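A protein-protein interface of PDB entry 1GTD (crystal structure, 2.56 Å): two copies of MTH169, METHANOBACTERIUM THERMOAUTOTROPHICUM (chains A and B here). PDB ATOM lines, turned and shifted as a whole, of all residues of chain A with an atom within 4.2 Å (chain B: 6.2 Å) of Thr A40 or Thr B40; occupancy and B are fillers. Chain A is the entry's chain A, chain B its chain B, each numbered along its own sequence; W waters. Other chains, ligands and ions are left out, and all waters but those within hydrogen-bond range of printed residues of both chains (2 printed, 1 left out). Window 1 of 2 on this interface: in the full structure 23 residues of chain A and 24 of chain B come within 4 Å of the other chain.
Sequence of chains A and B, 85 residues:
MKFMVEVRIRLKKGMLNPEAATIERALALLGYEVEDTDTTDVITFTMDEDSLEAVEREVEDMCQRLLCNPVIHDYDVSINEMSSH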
ATOM      1  N   ILE A   9     -21.406   7.830  14.405  1.00  0.00           N
ATOM      2  CA  ILE A   9     -21.002   6.948  15.488  1.00  0.00           C
ATOM      3  C   ILE A   9     -20.893   7.686  16.819  1.00  0.00           C
ATOM      4  O   ILE A   9     -20.149   8.661  16.934  1.00  0.00           O
ATOM      5  CB  ILE A   9     -19.640   6.313  15.141  1.00  0.00           C
ATOM      6  CG1 ILE A   9     -19.731   5.686  13.746  1.00  0.00           C
ATOM      7  CG2 ILE A   9     -19.250   5.282  16.186  1.00  0.00           C
ATOM      8  CD1 ILE A   9     -18.419   5.342  13.125  1.00  0.00           C
ATOM      9  N   ARG A  10     -21.644   7.226  17.819  1.00  0.00           N
ATOM     10  CA  ARG A  10     -21.615   7.842  19.145  1.00  0.00           C
ATOM     11  C   ARG A  10     -21.635   6.798  20.259  1.00  0.00           C
ATOM     12  O   ARG A  10     -22.420   5.864  20.213  1.00  0.00           O
ATOM     13  CB  ARG A  10     -22.802   8.790  19.316  1.00  0.00           C
ATOM     14  CG  ARG A  10     -22.729   9.623  20.596  1.00  0.00           C
ATOM     15  CD  ARG A  10     -23.675  10.797  20.530  1.00  0.00           C
ATOM     16  NE  ARG A  10     -25.063  10.354  20.471  1.00  0.00           N
ATOM     17  CZ  ARG A  10     -26.031  11.000  19.821  1.00  0.00           C
ATOM     18  NH1 ARG A  10     -25.763  12.125  19.164  1.00  0.00           N
ATOM     19  NH2 ARG A  10     -27.273  10.517  19.829  1.00  0.00           N
ATOM     20  N   THR A  39     -19.595  13.712  21.967  1.00  0.00           N
ATOM     21  CA  THR A  39     -18.943  13.776  20.666  1.00  0.00           C
ATOM     22  C   THR A  39     -19.475  12.703  19.742  1.00  0.00           C
ATOM     23  O   THR A  39     -19.747  11.575  20.156  1.00  0.00           O
ATOM     24  CB  THR A  39     -17.404  13.584  20.742  1.00  0.00           C
ATOM     25  OG1 THR A  39     -17.101  12.190  20.907  1.00  0.00           O
ATOM     26  CG2 THR A  39     -16.801  14.409  21.884  1.00  0.00           C
ATOM     27  N   THR A  40     -19.606  13.074  18.476  1.00  0.00           N
ATOM     28  CA  THR A  40     -20.091  12.184  17.445  1.00  0.00           C
ATOM     29  C   THR A  40     -19.089  12.206  16.303  1.00  0.00           C
ATOM     30  O   THR A  40     -18.543  13.248  15.970  1.00  0.00           O
ATOM     31  CB  THR A  40     -21.458  12.653  16.925  1.00  0.00           C
ATOM     32  OG1 THR A  40     -22.372  12.747  18.027  1.00  0.00           O
ATOM     33  CG2 THR A  40     -22.012  11.680  15.882  1.00  0.00           C
ATOM     34  N   ASP A  41     -18.842  11.042  15.721  1.00  0.00           N
ATOM     35  CA  ASP A  41     -17.911  10.918  14.613  1.00  0.00           C
ATOM     36  C   ASP A  41     -18.736  10.604  13.390  1.00  0.00           C
ATOM     37  O   ASP A  41     -19.498   9.645  13.394  1.00  0.00           O
ATOM     38  CB  ASP A  41     -16.918   9.784  14.871  1.00  0.00           C
ATOM     39  CG  ASP A  41     -15.895  10.139  15.937  1.00  0.00           C
ATOM     40  OD1 ASP A  41     -14.949  10.906  15.630  1.00  0.00           O
ATOM     41  OD2 ASP A  41     -16.043   9.663  17.088  1.00  0.00           O
ATOM     42  N   VAL A  42     -18.608  11.419  12.349  1.00  0.00           N
ATOM     43  CA  VAL A  42     -19.374  11.172  11.133  1.00  0.00           C
ATOM     44  C   VAL A  42     -18.465  10.832   9.965  1.00  0.00           C
ATOM     45  O   VAL A  42     -17.549  11.588   9.636  1.00  0.00           O
ATOM     46  CB  VAL A  42     -20.238  12.387  10.735  1.00  0.00           C
ATOM     47  CG1 VAL A  42     -21.041  12.057   9.468  1.00  0.00           C
ATOM     48  CG2 VAL A  42     -21.173  12.763  11.877  1.00  0.00           C
ATOM     49  N   ARG B   8     -19.929  21.439  14.628  1.00  0.00           N
ATOM     50  CA  ARG B   8     -19.463  20.451  13.659  1.00  0.00           C
ATOM     51  C   ARG B   8     -18.153  20.953  13.073  1.00  0.00           C
ATOM     52  O   ARG B   8     -18.069  22.085  12.606  1.00  0.00           O
ATOM     53  CB  ARG B   8     -20.520  20.245  12.580  1.00  0.00           C
ATOM     54  CG  ARG B   8     -21.879  19.885  13.171  1.00  0.00           C
ATOM     55  CD  ARG B   8     -22.903  19.611  12.099  1.00  0.00           C
ATOM     56  NE  ARG B   8     -22.586  18.392  11.361  1.00  0.00           N
ATOM     57  CZ  ARG B   8     -23.191  17.218  11.541  1.00  0.00           C
ATOM     58  NH1 ARG B   8     -24.164  17.096  12.444  1.00  0.00           N
ATOM     59  NH2 ARG B   8     -22.820  16.163  10.816  1.00  0.00           N
ATOM     60  N   ILE B   9     -17.126  20.112  13.120  1.00  0.00           N
ATOM     61  CA  ILE B   9     -15.800  20.480  12.641  1.00  0.00           C
ATOM     62  C   ILE B   9     -15.277  19.559  11.540  1.00  0.00           C
ATOM     63  O   ILE B   9     -15.247  18.343  11.699  1.00  0.00           O
ATOM     64  CB  ILE B   9     -14.824  20.479  13.821  1.00  0.00           C
ATOM     65  CG1 ILE B   9     -15.433  21.298  14.958  1.00  0.00           C
ATOM     66  CG2 ILE B   9     -13.499  21.092  13.423  1.00  0.00           C
ATOM     67  CD1 ILE B   9     -14.683  21.231  16.265  1.00  0.00           C
ATOM     68  N   ARG B  10     -14.855  20.147  10.423  1.00  0.00           N
ATOM     69  CA  ARG B  10     -14.339  19.359   9.309  1.00  0.00           C
ATOM     70  C   ARG B  10     -13.231  20.098   8.549  1.00  0.00           C
ATOM     71  O   ARG B  10     -13.351  21.283   8.248  1.00  0.00           O
ATOM     72  CB  ARG B  10     -15.485  18.997   8.366  1.00  0.00           C
ATOM     73  CG  ARG B  10     -15.097  18.044   7.255  1.00  0.00           C
ATOM     74  CD  ARG B  10     -16.322  17.616   6.475  1.00  0.00           C
ATOM     75  NE  ARG B  10     -17.059  18.774   5.973  1.00  0.00           N
ATOM     76  CZ  ARG B  10     -18.217  18.701   5.320  1.00  0.00           C
ATOM     77  NH1 ARG B  10     -18.779  17.518   5.086  1.00  0.00           N
ATOM     78  NH2 ARG B  10     -18.812  19.813   4.900  1.00  0.00           N
ATOM     79  N   ASN B  17      -6.581  14.165   5.259  1.00  0.00           N
ATOM     80  CA  ASN B  17      -7.334  13.691   6.408  1.00  0.00           C
ATOM     81  C   ASN B  17      -6.817  12.289   6.666  1.00  0.00           C
ATOM     82  O   ASN B  17      -7.280  11.324   6.059  1.00  0.00           O
ATOM     83  CB  ASN B  17      -8.826  13.657   6.099  1.00  0.00           C
ATOM     84  CG  ASN B  17      -9.658  13.238   7.295  1.00  0.00           C
ATOM     85  OD1 ASN B  17     -10.884  13.272   7.243  1.00  0.00           O
ATOM     86  ND2 ASN B  17      -8.996  12.843   8.379  1.00  0.00           N
ATOM     87  N   ASP B  38     -14.737  10.972   3.992  1.00  0.00           N
ATOM     88  CA  ASP B  38     -14.628  12.232   4.713  1.00  0.00           C
ATOM     89  C   ASP B  38     -15.004  11.995   6.179  1.00  0.00           C
ATOM     90  O   ASP B  38     -15.768  11.071   6.493  1.00  0.00           O
ATOM     91  CB  ASP B  38     -15.584  13.239   4.076  1.00  0.00           C
ATOM     92  CG  ASP B  38     -15.076  14.657   4.141  1.00  0.00           C
ATOM     93  OD1 ASP B  38     -15.783  15.554   3.616  1.00  0.00           O
ATOM     94  OD2 ASP B  38     -13.980  14.876   4.710  1.00  0.00           O
ATOM     95  N   THR B  39     -14.482  12.836   7.067  1.00  0.00           N
ATOM     96  CA  THR B  39     -14.742  12.708   8.502  1.00  0.00           C
ATOM     97  C   THR B  39     -15.144  14.042   9.133  1.00  0.00           C
ATOM     98  O   THR B  39     -14.544  15.080   8.852  1.00  0.00           O
ATOM     99  CB  THR B  39     -13.469  12.167   9.230  1.00  0.00           C
ATOM    100  OG1 THR B  39     -13.559  10.742   9.382  1.00  0.00           O
ATOM    101  CG2 THR B  39     -13.277  12.841  10.584  1.00  0.00           C
ATOM    102  N   THR B  40     -16.160  14.007   9.987  1.00  0.00           N
ATOM    103  CA  THR B  40     -16.623  15.207  10.666  1.00  0.00           C
ATOM    104  C   THR B  40     -16.682  14.905  12.150  1.00  0.00           C
ATOM    105  O   THR B  40     -17.050  13.795  12.556  1.00  0.00           O
ATOM    106  CB  THR B  40     -18.033  15.616  10.209  1.00  0.00           C
ATOM    107  OG1 THR B  40     -18.061  15.753   8.782  1.00  0.00           O
ATOM    108  CG2 THR B  40     -18.423  16.941  10.844  1.00  0.00           C
ATOM    109  N   ASP B  41     -16.313  15.884  12.961  1.00  0.00           N
ATOM    110  CA  ASP B  41     -16.345  15.713  14.402  1.00  0.00           C
ATOM    111  C   ASP B  41     -17.443  16.604  14.919  1.00  0.00           C
ATOM    112  O   ASP B  41     -17.489  17.782  14.589  1.00  0.00           O
ATOM    113  CB  ASP B  41     -15.013  16.117  15.019  1.00  0.00           C
ATOM    114  CG  ASP B  41     -13.865  15.318  14.463  1.00  0.00           C
ATOM    115  OD1 ASP B  41     -13.009  15.911  13.761  1.00  0.00           O
ATOM    116  OD2 ASP B  41     -13.835  14.087  14.710  1.00  0.00           O
ATOM    117  N   VAL B  42     -18.337  16.047  15.721  1.00  0.00           N
ATOM    118  CA  VAL B  42     -19.424  16.848  16.247  1.00  0.00           C
ATOM    119  C   VAL B  42     -19.376  16.894  17.763  1.00  0.00           C
ATOM    120  O   VAL B  42     -19.339  15.862  18.429  1.00  0.00           O
ATOM    121  CB  VAL B  42     -20.779  16.299  15.788  1.00  0.00           C
ATOM    122  CG1 VAL B  42     -21.893  17.257  16.196  1.00  0.00           C
ATOM    123  CG2 VAL B  42     -20.750  16.078  14.275  1.00  0.00           C
ATOM    124  N   ILE B  43     -19.353  18.111  18.291  1.00  0.00           N
ATOM    125  CA  ILE B  43     -19.324  18.323  19.721  1.00  0.00           C
ATOM    126  C   ILE B  43     -20.646  18.959  20.094  1.00  0.00           C
ATOM    127  O   ILE B  43     -21.046  19.948  19.482  1.00  0.00           O
ATOM    128  CB  ILE B  43     -18.208  19.275  20.113  1.00  0.00           C
ATOM    129  CG1 ILE B  43     -16.897  18.793  19.500  1.00  0.00           C
ATOM    130  CG2 ILE B  43     -18.110  19.351  21.626  1.00  0.00           C
ATOM    131  CD1 ILE B  43     -15.735  19.723  19.734  1.00  0.00           C
ATOM    132  N   THR B  44     -21.328  18.385  21.083  1.00  0.00           N
ATOM    133  CA  THR B  44     -22.603  18.922  21.534  1.00  0.00           C
ATOM    134  C   THR B  44     -22.510  19.182  23.036  1.00  0.00           C
ATOM    135  O   THR B  44     -21.739  18.533  23.733  1.00  0.00           O
ATOM    136  CB  THR B  44     -23.759  17.934  21.267  1.00  0.00           C
ATOM    137  OG1 THR B  44     -23.592  17.313  19.983  1.00  0.00           O
ATOM    138  CG2 THR B  44     -25.076  18.676  21.258  1.00  0.00           C
HETATM  139  O   HOH W   1     -22.005  15.303  19.341  1.00  0.00           O
HETATM  140  O   HOH W   2     -15.267  11.182  12.479  1.00  0.00           O
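Among the printed residues, pairs that only touch across the chains: Thr A39 with Val B42 (3.1 Å), Val A42 with Thr B39 (3.2 Å), Asp A41 with Thr B40 (3.6 Å), Val A42 with Asp B38 (3.6 Å), Thr A40 with Asp B41 (3.7 Å), Thr A40 with Thr B40 (3.8 Å) and Val A42 with Arg B8 (3.9 Å).
Hydrophobic or aromatic side chains of chain B within 4 Å of the printed part of chain A: Val B42.
Water W1 lies within hydrogen-bond range of OG1 of Thr B44 (2.6 Å), O of Val B42 (2.9 Å) and OG1 of Thr A40 (2.9 Å). Water W2 lies within hydrogen-bond range of O of Thr B40 (3.2 Å), OD1 of Asp A41 (3.2 Å) and N of Val A42 (3.4 Å).
The backbone NH of Thr A40 sits at hydrogen-bond distance from the backbone carbonyl oxygen of Val B42. The backbone NH (N) of Thr B40 is in hydrogen-bond range of the backbone carbonyl oxygen (O) of Val A42, 2.8 Å away. The side-chain carboxylate (OD1) of Asp A41 lies close to the side-chain carboxylate (OD2) of Asp B41.
Of chain B, only Thr B40 (3.8 Å), Asp B41 (3.7 Å) and Val B42 (2.8 Å) come within 4 Å of Thr A40. Of the printed residues of chain A, Thr B39 touches Val A42. Printed residues of chain A within 4 Å of Val B42: Thr A39 and Thr A40. Of the printed residues of chain A, Arg B8 touches Val A42. Asn B17 touches none of the printed residues of chain A. Ile A9 touches none of the printed residues of chain B.
Thr A39 touches Val B42, and with the chains exchanged Val A42 touches Thr B39. Thr A40 touches Asp B41, and with the chains exchanged Asp A41 touches Thr B40. Thr A40 touches Val B42, and with the chains exchanged Val A42 touches Thr B40. Asp A41 touches its own counterpart, Asp B41. 6 positions are printed for both chains. Of the 10 pairs that touch across the chains among the printed residues, 8 have their exchanged pair printed and touching as well.
N of Ile A9 is in hydrogen-bond range of O of Asp A41 (2.8 Å). The backbone carbonyl oxygen (O) of Asp B41 is in hydrogen-bond range of the backbone NH (N) of Ile B9 (2.8 Å). NH1 of Arg B10 is in salt-bridge range of OD1 of Asp B38.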
